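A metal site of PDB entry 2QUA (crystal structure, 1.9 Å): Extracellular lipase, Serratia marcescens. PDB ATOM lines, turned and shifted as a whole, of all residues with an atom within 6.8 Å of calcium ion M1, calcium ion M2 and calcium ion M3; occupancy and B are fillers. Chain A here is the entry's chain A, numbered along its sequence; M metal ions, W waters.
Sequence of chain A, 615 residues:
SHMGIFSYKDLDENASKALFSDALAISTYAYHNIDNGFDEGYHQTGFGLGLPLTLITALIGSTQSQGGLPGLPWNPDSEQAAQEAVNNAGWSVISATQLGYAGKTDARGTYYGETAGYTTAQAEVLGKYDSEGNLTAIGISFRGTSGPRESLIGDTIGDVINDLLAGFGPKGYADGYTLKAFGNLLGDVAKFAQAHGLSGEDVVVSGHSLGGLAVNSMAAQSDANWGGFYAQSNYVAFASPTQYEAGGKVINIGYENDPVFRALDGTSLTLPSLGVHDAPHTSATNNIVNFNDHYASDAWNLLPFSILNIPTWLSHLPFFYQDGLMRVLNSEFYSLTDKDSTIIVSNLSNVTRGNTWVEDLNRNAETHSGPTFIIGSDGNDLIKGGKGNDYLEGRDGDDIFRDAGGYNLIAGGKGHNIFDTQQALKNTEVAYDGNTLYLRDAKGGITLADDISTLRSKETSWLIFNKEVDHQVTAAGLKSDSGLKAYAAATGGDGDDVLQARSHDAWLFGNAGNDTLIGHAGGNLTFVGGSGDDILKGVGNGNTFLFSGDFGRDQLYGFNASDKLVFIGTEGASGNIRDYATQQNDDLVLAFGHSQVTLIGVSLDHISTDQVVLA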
ATOM      1  N   GLY A 492     -14.276   1.183   2.564  1.00  0.00           N
ATOM      2  CA  GLY A 492     -14.755  -0.191   2.356  1.00  0.00           C
ATOM      3  C   GLY A 492     -13.923  -0.919   1.308  1.00  0.00           C
ATOM      4  O   GLY A 492     -12.898  -0.406   0.849  1.00  0.00           O
ATOM      5  N   GLY A 493     -14.375  -2.120   0.939  1.00  0.00           N
ATOM      6  CA  GLY A 493     -13.717  -2.936  -0.077  1.00  0.00           C
ATOM      7  C   GLY A 493     -14.687  -3.403  -1.152  1.00  0.00           C
ATOM      8  O   GLY A 493     -15.698  -2.751  -1.408  1.00  0.00           O
ATOM      9  N   ASP A 494     -14.385  -4.555  -1.758  1.00  0.00           N
ATOM     10  CA  ASP A 494     -15.192  -5.136  -2.829  1.00  0.00           C
ATOM     11  C   ASP A 494     -16.612  -5.509  -2.395  1.00  0.00           C
ATOM     12  O   ASP A 494     -17.515  -5.638  -3.221  1.00  0.00           O
ATOM     13  CB  ASP A 494     -14.512  -6.378  -3.391  1.00  0.00           C
ATOM     14  CG  ASP A 494     -13.282  -6.054  -4.227  1.00  0.00           C
ATOM     15  OD1 ASP A 494     -13.188  -4.905  -4.712  1.00  0.00           O
ATOM     16  OD2 ASP A 494     -12.422  -6.946  -4.407  1.00  0.00           O
ATOM     17  N   GLY A 495     -16.778  -5.697  -1.089  1.00  0.00           N
ATOM     18  CA  GLY A 495     -18.061  -6.159  -0.547  1.00  0.00           C
ATOM     19  C   GLY A 495     -19.104  -5.066  -0.434  1.00  0.00           C
ATOM     20  O   GLY A 495     -18.832  -3.888  -0.669  1.00  0.00           O
ATOM     21  N   ASP A 496     -20.309  -5.470  -0.073  1.00  0.00           N
ATOM     22  CA  ASP A 496     -21.400  -4.570   0.203  1.00  0.00           C
ATOM     23  C   ASP A 496     -21.191  -4.103   1.636  1.00  0.00           C
ATOM     24  O   ASP A 496     -21.639  -4.748   2.584  1.00  0.00           O
ATOM     25  CB  ASP A 496     -22.740  -5.302   0.038  1.00  0.00           C
ATOM     26  CG  ASP A 496     -22.905  -5.915  -1.357  1.00  0.00           C
ATOM     27  OD1 ASP A 496     -22.210  -5.473  -2.301  1.00  0.00           O
ATOM     28  OD2 ASP A 496     -23.728  -6.830  -1.514  1.00  0.00           O
ATOM     29  N   ASP A 497     -20.500  -2.976   1.781  1.00  0.00           N
ATOM     30  CA  ASP A 497     -20.076  -2.487   3.089  1.00  0.00           C
ATOM     31  C   ASP A 497     -21.089  -1.541   3.735  1.00  0.00           C
ATOM     32  O   ASP A 497     -21.751  -0.752   3.052  1.00  0.00           O
ATOM     33  CB  ASP A 497     -18.744  -1.754   2.944  1.00  0.00           C
ATOM     34  CG  ASP A 497     -17.690  -2.601   2.258  1.00  0.00           C
ATOM     35  OD1 ASP A 497     -17.403  -3.698   2.774  1.00  0.00           O
ATOM     36  OD2 ASP A 497     -17.161  -2.170   1.215  1.00  0.00           O
ATOM     37  N   LEU A 499     -20.826   1.566   6.076  1.00  0.00           N
ATOM     38  CA  LEU A 499     -19.861   2.519   6.612  1.00  0.00           C
ATOM     39  C   LEU A 499     -20.528   3.627   7.415  1.00  0.00           C
ATOM     40  O   LEU A 499     -21.231   4.472   6.848  1.00  0.00           O
ATOM     41  CB  LEU A 499     -19.042   3.144   5.474  1.00  0.00           C
ATOM     42  CG  LEU A 499     -18.267   2.161   4.603  1.00  0.00           C
ATOM     43  CD1 LEU A 499     -17.482   2.887   3.520  1.00  0.00           C
ATOM     44  CD2 LEU A 499     -17.358   1.338   5.487  1.00  0.00           C
ATOM     45  N   PHE A 509     -15.621   6.073   1.558  1.00  0.00           N
ATOM     46  CA  PHE A 509     -15.402   5.402   0.283  1.00  0.00           C
ATOM     47  C   PHE A 509     -16.003   3.996   0.327  1.00  0.00           C
ATOM     48  O   PHE A 509     -15.477   3.119   1.015  1.00  0.00           O
ATOM     49  CB  PHE A 509     -13.905   5.286   0.004  1.00  0.00           C
ATOM     50  CG  PHE A 509     -13.178   6.611  -0.090  1.00  0.00           C
ATOM     51  CD1 PHE A 509     -13.459   7.510  -1.117  1.00  0.00           C
ATOM     52  CD2 PHE A 509     -12.215   6.953   0.848  1.00  0.00           C
ATOM     53  CE1 PHE A 509     -12.769   8.730  -1.200  1.00  0.00           C
ATOM     54  CE2 PHE A 509     -11.527   8.159   0.768  1.00  0.00           C
ATOM     55  CZ  PHE A 509     -11.815   9.037  -0.255  1.00  0.00           C
ATOM     56  N   GLY A 510     -17.104   3.783  -0.387  1.00  0.00           N
ATOM     57  CA  GLY A 510     -17.722   2.471  -0.440  1.00  0.00           C
ATOM     58  C   GLY A 510     -16.912   1.512  -1.302  1.00  0.00           C
ATOM     59  O   GLY A 510     -16.856   0.328  -1.008  1.00  0.00           O
ATOM     60  N   ASN A 511     -16.288   2.045  -2.358  1.00  0.00           N
ATOM     61  CA  ASN A 511     -15.583   1.225  -3.358  1.00  0.00           C
ATOM     62  C   ASN A 511     -16.571   0.293  -4.057  1.00  0.00           C
ATOM     63  O   ASN A 511     -17.754   0.619  -4.143  1.00  0.00           O
ATOM     64  CB  ASN A 511     -14.380   0.471  -2.726  1.00  0.00           C
ATOM     65  CG  ASN A 511     -13.180   1.408  -2.448  1.00  0.00           C
ATOM     66  OD1 ASN A 511     -12.882   2.290  -3.240  1.00  0.00           O
ATOM     67  ND2 ASN A 511     -12.499   1.208  -1.322  1.00  0.00           N
ATOM     68  N   ALA A 512     -16.125  -0.840  -4.558  1.00  0.00           N
ATOM     69  CA  ALA A 512     -17.028  -1.722  -5.311  1.00  0.00           C
ATOM     70  C   ALA A 512     -18.130  -2.295  -4.434  1.00  0.00           C
ATOM     71  O   ALA A 512     -18.050  -2.268  -3.201  1.00  0.00           O
ATOM     72  CB  ALA A 512     -16.255  -2.840  -5.985  1.00  0.00           C
ATOM     73  N   GLY A 513     -19.172  -2.825  -5.068  1.00  0.00           N
ATOM     74  CA  GLY A 513     -20.280  -3.407  -4.323  1.00  0.00           C
ATOM     75  C   GLY A 513     -21.313  -2.365  -3.929  1.00  0.00           C
ATOM     76  O   GLY A 513     -21.141  -1.154  -4.161  1.00  0.00           O
ATOM     77  N   ASN A 514     -22.383  -2.843  -3.328  1.00  0.00           N
ATOM     78  CA  ASN A 514     -23.509  -1.996  -2.940  1.00  0.00           C
ATOM     79  C   ASN A 514     -23.376  -1.604  -1.467  1.00  0.00           C
ATOM     80  O   ASN A 514     -23.692  -2.381  -0.567  1.00  0.00           O
ATOM     81  CB  ASN A 514     -24.830  -2.707  -3.264  1.00  0.00           C
ATOM     82  CG  ASN A 514     -24.967  -3.009  -4.758  1.00  0.00           C
ATOM     83  OD1 ASN A 514     -24.144  -2.588  -5.580  1.00  0.00           O
ATOM     84  ND2 ASN A 514     -26.022  -3.729  -5.112  1.00  0.00           N
ATOM     85  N   ASP A 515     -22.899  -0.388  -1.253  1.00  0.00           N
ATOM     86  CA  ASP A 515     -22.527   0.085   0.073  1.00  0.00           C
ATOM     87  C   ASP A 515     -23.544   1.034   0.697  1.00  0.00           C
ATOM     88  O   ASP A 515     -24.275   1.745  -0.017  1.00  0.00           O
ATOM     89  CB  ASP A 515     -21.189   0.830  -0.054  1.00  0.00           C
ATOM     90  CG  ASP A 515     -20.097  -0.025  -0.702  1.00  0.00           C
ATOM     91  OD1 ASP A 515     -19.759  -1.067  -0.131  1.00  0.00           O
ATOM     92  OD2 ASP A 515     -19.586   0.363  -1.779  1.00  0.00           O
ATOM     93  N   LEU A 517     -23.502   4.215   3.171  1.00  0.00           N
ATOM     94  CA  LEU A 517     -22.666   5.254   3.776  1.00  0.00           C
ATOM     95  C   LEU A 517     -23.517   6.184   4.630  1.00  0.00           C
ATOM     96  O   LEU A 517     -24.442   6.831   4.117  1.00  0.00           O
ATOM     97  CB  LEU A 517     -21.937   6.069   2.697  1.00  0.00           C
ATOM     98  CG  LEU A 517     -20.733   5.480   1.958  1.00  0.00           C
ATOM     99  CD1 LEU A 517     -21.011   4.089   1.425  1.00  0.00           C
ATOM    100  CD2 LEU A 517     -20.294   6.405   0.809  1.00  0.00           C
ATOM    101  N   VAL A 528     -18.569   9.029  -1.190  1.00  0.00           N
ATOM    102  CA  VAL A 528     -18.191   8.481  -2.476  1.00  0.00           C
ATOM    103  C   VAL A 528     -18.626   7.020  -2.514  1.00  0.00           C
ATOM    104  O   VAL A 528     -17.910   6.141  -2.001  1.00  0.00           O
ATOM    105  CB  VAL A 528     -16.682   8.538  -2.660  1.00  0.00           C
ATOM    106  CG1 VAL A 528     -16.326   8.199  -4.112  1.00  0.00           C
ATOM    107  CG2 VAL A 528     -16.142   9.902  -2.237  1.00  0.00           C
ATOM    108  N   GLY A 529     -19.795   6.734  -3.085  1.00  0.00           N
ATOM    109  CA  GLY A 529     -20.287   5.343  -3.053  1.00  0.00           C
ATOM    110  C   GLY A 529     -19.436   4.413  -3.907  1.00  0.00           C
ATOM    111  O   GLY A 529     -19.321   3.208  -3.633  1.00  0.00           O
ATOM    112  N   GLY A 530     -18.814   4.997  -4.935  1.00  0.00           N
ATOM    113  CA  GLY A 530     -17.960   4.276  -5.858  1.00  0.00           C
ATOM    114  C   GLY A 530     -18.831   3.495  -6.827  1.00  0.00           C
ATOM    115  O   GLY A 530     -20.015   3.788  -6.967  1.00  0.00           O
ATOM    116  N   SER A 531     -18.252   2.511  -7.482  1.00  0.00           N
ATOM    117  CA  SER A 531     -19.042   1.656  -8.353  1.00  0.00           C
ATOM    118  C   SER A 531     -20.029   0.856  -7.502  1.00  0.00           C
ATOM    119  O   SER A 531     -19.929   0.831  -6.266  1.00  0.00           O
ATOM    120  CB  SER A 531     -18.150   0.730  -9.183  1.00  0.00           C
ATOM    121  OG  SER A 531     -17.611  -0.294  -8.376  1.00  0.00           O
ATOM    122  N   GLY A 532     -20.983   0.214  -8.162  1.00  0.00           N
ATOM    123  CA  GLY A 532     -22.079  -0.475  -7.474  1.00  0.00           C
ATOM    124  C   GLY A 532     -23.188   0.499  -7.103  1.00  0.00           C
ATOM    125  O   GLY A 532     -23.082   1.730  -7.255  1.00  0.00           O
ATOM    126  N   ASP A 533     -24.275  -0.059  -6.600  1.00  0.00           N
ATOM    127  CA  ASP A 533     -25.465   0.715  -6.285  1.00  0.00           C
ATOM    128  C   ASP A 533     -25.512   0.992  -4.805  1.00  0.00           C
ATOM    129  O   ASP A 533     -25.760   0.087  -4.011  1.00  0.00           O
ATOM    130  CB  ASP A 533     -26.709  -0.032  -6.725  1.00  0.00           C
ATOM    131  CG  ASP A 533     -26.685  -0.359  -8.206  1.00  0.00           C
ATOM    132  OD1 ASP A 533     -25.951   0.313  -8.962  1.00  0.00           O
ATOM    133  OD2 ASP A 533     -27.413  -1.287  -8.629  1.00  0.00           O
ATOM    134  N   ASP A 534     -25.271   2.255  -4.453  1.00  0.00           N
ATOM    135  CA  ASP A 534     -25.015   2.640  -3.057  1.00  0.00           C
ATOM    136  C   ASP A 534     -26.125   3.497  -2.433  1.00  0.00           C
ATOM    137  O   ASP A 534     -26.853   4.210  -3.105  1.00  0.00           O
ATOM    138  CB  ASP A 534     -23.673   3.390  -2.968  1.00  0.00           C
ATOM    139  CG  ASP A 534     -22.518   2.615  -3.607  1.00  0.00           C
ATOM    140  OD1 ASP A 534     -22.119   1.563  -3.068  1.00  0.00           O
ATOM    141  OD2 ASP A 534     -22.009   3.037  -4.661  1.00  0.00           O
ATOM    142  N   LEU A 536     -26.734   6.501   0.247  1.00  0.00           N
ATOM    143  CA  LEU A 536     -26.010   7.628   0.840  1.00  0.00           C
ATOM    144  C   LEU A 536     -26.897   8.405   1.809  1.00  0.00           C
ATOM    145  O   LEU A 536     -27.840   9.098   1.396  1.00  0.00           O
ATOM    146  CB  LEU A 536     -25.479   8.581  -0.242  1.00  0.00           C
ATOM    147  CG  LEU A 536     -24.916   7.884  -1.483  1.00  0.00           C
ATOM    148  CD1 LEU A 536     -24.738   8.910  -2.643  1.00  0.00           C
ATOM    149  CD2 LEU A 536     -23.605   7.124  -1.178  1.00  0.00           C
ATOM    150  N   PHE A 547     -19.542  11.708  -7.464  1.00  0.00           N
ATOM    151  CA  PHE A 547     -19.824  10.652  -8.437  1.00  0.00           C
ATOM    152  C   PHE A 547     -18.916  10.824  -9.635  1.00  0.00           C
ATOM    153  O   PHE A 547     -18.810  11.940 -10.163  1.00  0.00           O
ATOM    154  CB  PHE A 547     -21.267  10.755  -8.934  1.00  0.00           C
ATOM    155  CG  PHE A 547     -22.269  10.878  -7.825  1.00  0.00           C
ATOM    156  CD1 PHE A 547     -22.852   9.742  -7.295  1.00  0.00           C
ATOM    157  CD2 PHE A 547     -22.610  12.120  -7.307  1.00  0.00           C
ATOM    158  CE1 PHE A 547     -23.783   9.842  -6.245  1.00  0.00           C
ATOM    159  CE2 PHE A 547     -23.541  12.235  -6.251  1.00  0.00           C
ATOM    160  CZ  PHE A 547     -24.131  11.091  -5.729  1.00  0.00           C
ATOM    161  N   ASP A 550     -18.496   5.480 -14.310  1.00  0.00           N
ATOM    162  CA  ASP A 550     -19.696   4.680 -14.155  1.00  0.00           C
ATOM    163  C   ASP A 550     -19.947   4.428 -12.667  1.00  0.00           C
ATOM    164  O   ASP A 550     -19.444   3.460 -12.095  1.00  0.00           O
ATOM    165  CB  ASP A 550     -19.593   3.381 -14.955  1.00  0.00           C
ATOM    166  CG  ASP A 550     -19.411   3.645 -16.464  1.00  0.00           C
ATOM    167  OD1 ASP A 550     -20.250   4.384 -17.041  1.00  0.00           O
ATOM    168  OD2 ASP A 550     -18.436   3.126 -17.059  1.00  0.00           O
ATOM    169  N   PHE A 551     -20.730   5.303 -12.041  1.00  0.00           N
ATOM    170  CA  PHE A 551     -20.917   5.241 -10.601  1.00  0.00           C
ATOM    171  C   PHE A 551     -22.142   4.412 -10.163  1.00  0.00           C
ATOM    172  O   PHE A 551     -22.509   4.452  -9.005  1.00  0.00           O
ATOM    173  CB  PHE A 551     -20.947   6.662  -9.986  1.00  0.00           C
ATOM    174  CG  PHE A 551     -22.069   7.519 -10.499  1.00  0.00           C
ATOM    175  CD1 PHE A 551     -21.882   8.319 -11.636  1.00  0.00           C
ATOM    176  CD2 PHE A 551     -23.317   7.543  -9.860  1.00  0.00           C
ATOM    177  CE1 PHE A 551     -22.916   9.114 -12.124  1.00  0.00           C
ATOM    178  CE2 PHE A 551     -24.357   8.331 -10.348  1.00  0.00           C
ATOM    179  CZ  PHE A 551     -24.164   9.123 -11.482  1.00  0.00           C
ATOM    180  N   GLY A 552     -22.748   3.664 -11.079  1.00  0.00           N
ATOM    181  CA  GLY A 552     -23.904   2.809 -10.741  1.00  0.00           C
ATOM    182  C   GLY A 552     -25.148   3.602 -10.385  1.00  0.00           C
ATOM    183  O   GLY A 552     -25.268   4.772 -10.744  1.00  0.00           O
ATOM    184  N   ARG A 553     -26.083   2.980  -9.663  1.00  0.00           N
ATOM    185  CA  ARG A 553     -27.334   3.655  -9.383  1.00  0.00           C
ATOM    186  C   ARG A 553     -27.532   3.889  -7.890  1.00  0.00           C
ATOM    187  O   ARG A 553     -27.872   2.957  -7.163  1.00  0.00           O
ATOM    188  CB  ARG A 553     -28.501   2.827  -9.941  1.00  0.00           C
ATOM    189  CG  ARG A 553     -28.367   2.513 -11.443  1.00  0.00           C
ATOM    190  CD  ARG A 553     -29.673   1.918 -12.020  1.00  0.00           C
ATOM    191  NE  ARG A 553     -29.461   1.337 -13.348  1.00  0.00           N
ATOM    192  CZ  ARG A 553     -29.360   2.036 -14.491  1.00  0.00           C
ATOM    193  NH1 ARG A 553     -29.442   3.369 -14.482  1.00  0.00           N
ATOM    194  NH2 ARG A 553     -29.176   1.401 -15.645  1.00  0.00           N
ATOM    195  N   ASP A 554     -27.336   5.122  -7.453  1.00  0.00           N
ATOM    196  CA  ASP A 554     -27.326   5.449  -6.031  1.00  0.00           C
ATOM    197  C   ASP A 554     -28.671   6.027  -5.553  1.00  0.00           C
ATOM    198  O   ASP A 554     -29.429   6.582  -6.347  1.00  0.00           O
ATOM    199  CB  ASP A 554     -26.246   6.499  -5.751  1.00  0.00           C
ATOM    200  CG  ASP A 554     -24.793   5.936  -5.735  1.00  0.00           C
ATOM    201  OD1 ASP A 554     -24.478   4.837  -6.269  1.00  0.00           O
ATOM    202  OD2 ASP A 554     -23.937   6.631  -5.140  1.00  0.00           O
ATOM    203  N   GLN A 596     -27.019   6.697 -12.146  1.00  0.00           N
ATOM    204  CA  GLN A 596     -28.026   7.676 -11.796  1.00  0.00           C
ATOM    205  C   GLN A 596     -28.001   7.890 -10.325  1.00  0.00           C
ATOM    206  O   GLN A 596     -27.460   7.061  -9.584  1.00  0.00           O
ATOM    207  CB  GLN A 596     -29.426   7.198 -12.224  1.00  0.00           C
ATOM    208  CG  GLN A 596     -30.025   6.153 -11.304  1.00  0.00           C
ATOM    209  CD  GLN A 596     -31.385   5.659 -11.765  1.00  0.00           C
ATOM    210  OE1 GLN A 596     -31.593   5.379 -12.952  1.00  0.00           O
ATOM    211  NE2 GLN A 596     -32.333   5.543 -10.832  1.00  0.00           N
HETATM  212 CA    CA M   1     -17.760  -1.812  -0.982  1.00  0.00          CA
HETATM  213 CA    CA M   2     -20.029   0.967  -3.954  1.00  0.00          CA
HETATM  214 CA    CA M   3     -22.349   3.920  -6.776  1.00  0.00          CA
HETATM  215  O   HOH W   1     -21.747   6.111  -6.218  1.00  0.00           O
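The backbone carbonyl oxygen (O) of Gly 492 is in hydrogen-bond range of the side-chain amide nitrogen (ND2) of Asn 511, at 2.7 Å. The backbone NH of Gly 510 lies within hydrogen-bond range of the backbone carbonyl oxygen of Val 528 (3.0 Å). O of Gln 596 sits at hydrogen-bond distance from N of Asp 554, 2.9 Å away.
Seven residues have an atom within 4 Å of calcium ion M1: Gly 493, Gly 495, Asp 497, Gly 510, Asn 511, Ala 512 and Asp 515. The nearest printed residue that does not touch calcium ion M1 is Asp 494 (4.1 Å).
Seven residues have an atom within 4 Å of calcium ion M2: Asn 511, Ala 512, Gly 513, Asp 515, Gly 529, Ser 531 and Asp 534. Along chain A the residues within 4 Å of calcium ion M2 span positions 511 to 534.
The nearest printed residue that does not touch calcium ion M3 is Gly 529 (4.1 Å).
Calcium ion M1 is bound by the backbone carbonyl oxygen of Ala 512 (2.3 Å), the side-chain carboxylate of Asp 515 (2.3 Å), the side-chain carboxylate of Asp 497 (2.3 Å), the backbone carbonyl oxygen of Gly 493 (2.3 Å), the backbone carbonyl oxygen of Gly 510 (2.3 Å) and the backbone carbonyl oxygen of Gly 495 (2.4 Å). Calcium ion M1 has six donor atoms within binding distance. Slightly farther from calcium ion M1 lies the side-chain carboxylate (OD2) of Asp 515 (2.9 Å).
Calcium ion M2 is bound by OD2 of Asp 515 (2.3 Å), O of Asn 511 (2.3 Å), O of Ser 531 (2.3 Å), OD1 of Asp 534 (2.3 Å), O of Gly 529 (2.4 Å) and O of Gly 513 (2.4 Å). Calcium ion M2 has six donor atoms within binding distance. Slightly farther from calcium ion M2 lies the side-chain carboxylate (OD2) of Asp 534 (3.0 Å).
Calcium ion M3 is bound by the backbone carbonyl oxygen of Phe 551 (2.3 Å), the side-chain carboxylate of Asp 534 (2.3 Å), water W1 (2.3 Å), the backbone carbonyl oxygen of Gly 530 (2.3 Å), the backbone carbonyl oxygen of Gly 532 (2.4 Å) and the side-chain carboxylate of Asp 554 (2.4 Å).
Water W1 bridges OD2 of Asp 554 (2.5 Å) and N of Gly 530 (3.4 Å).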
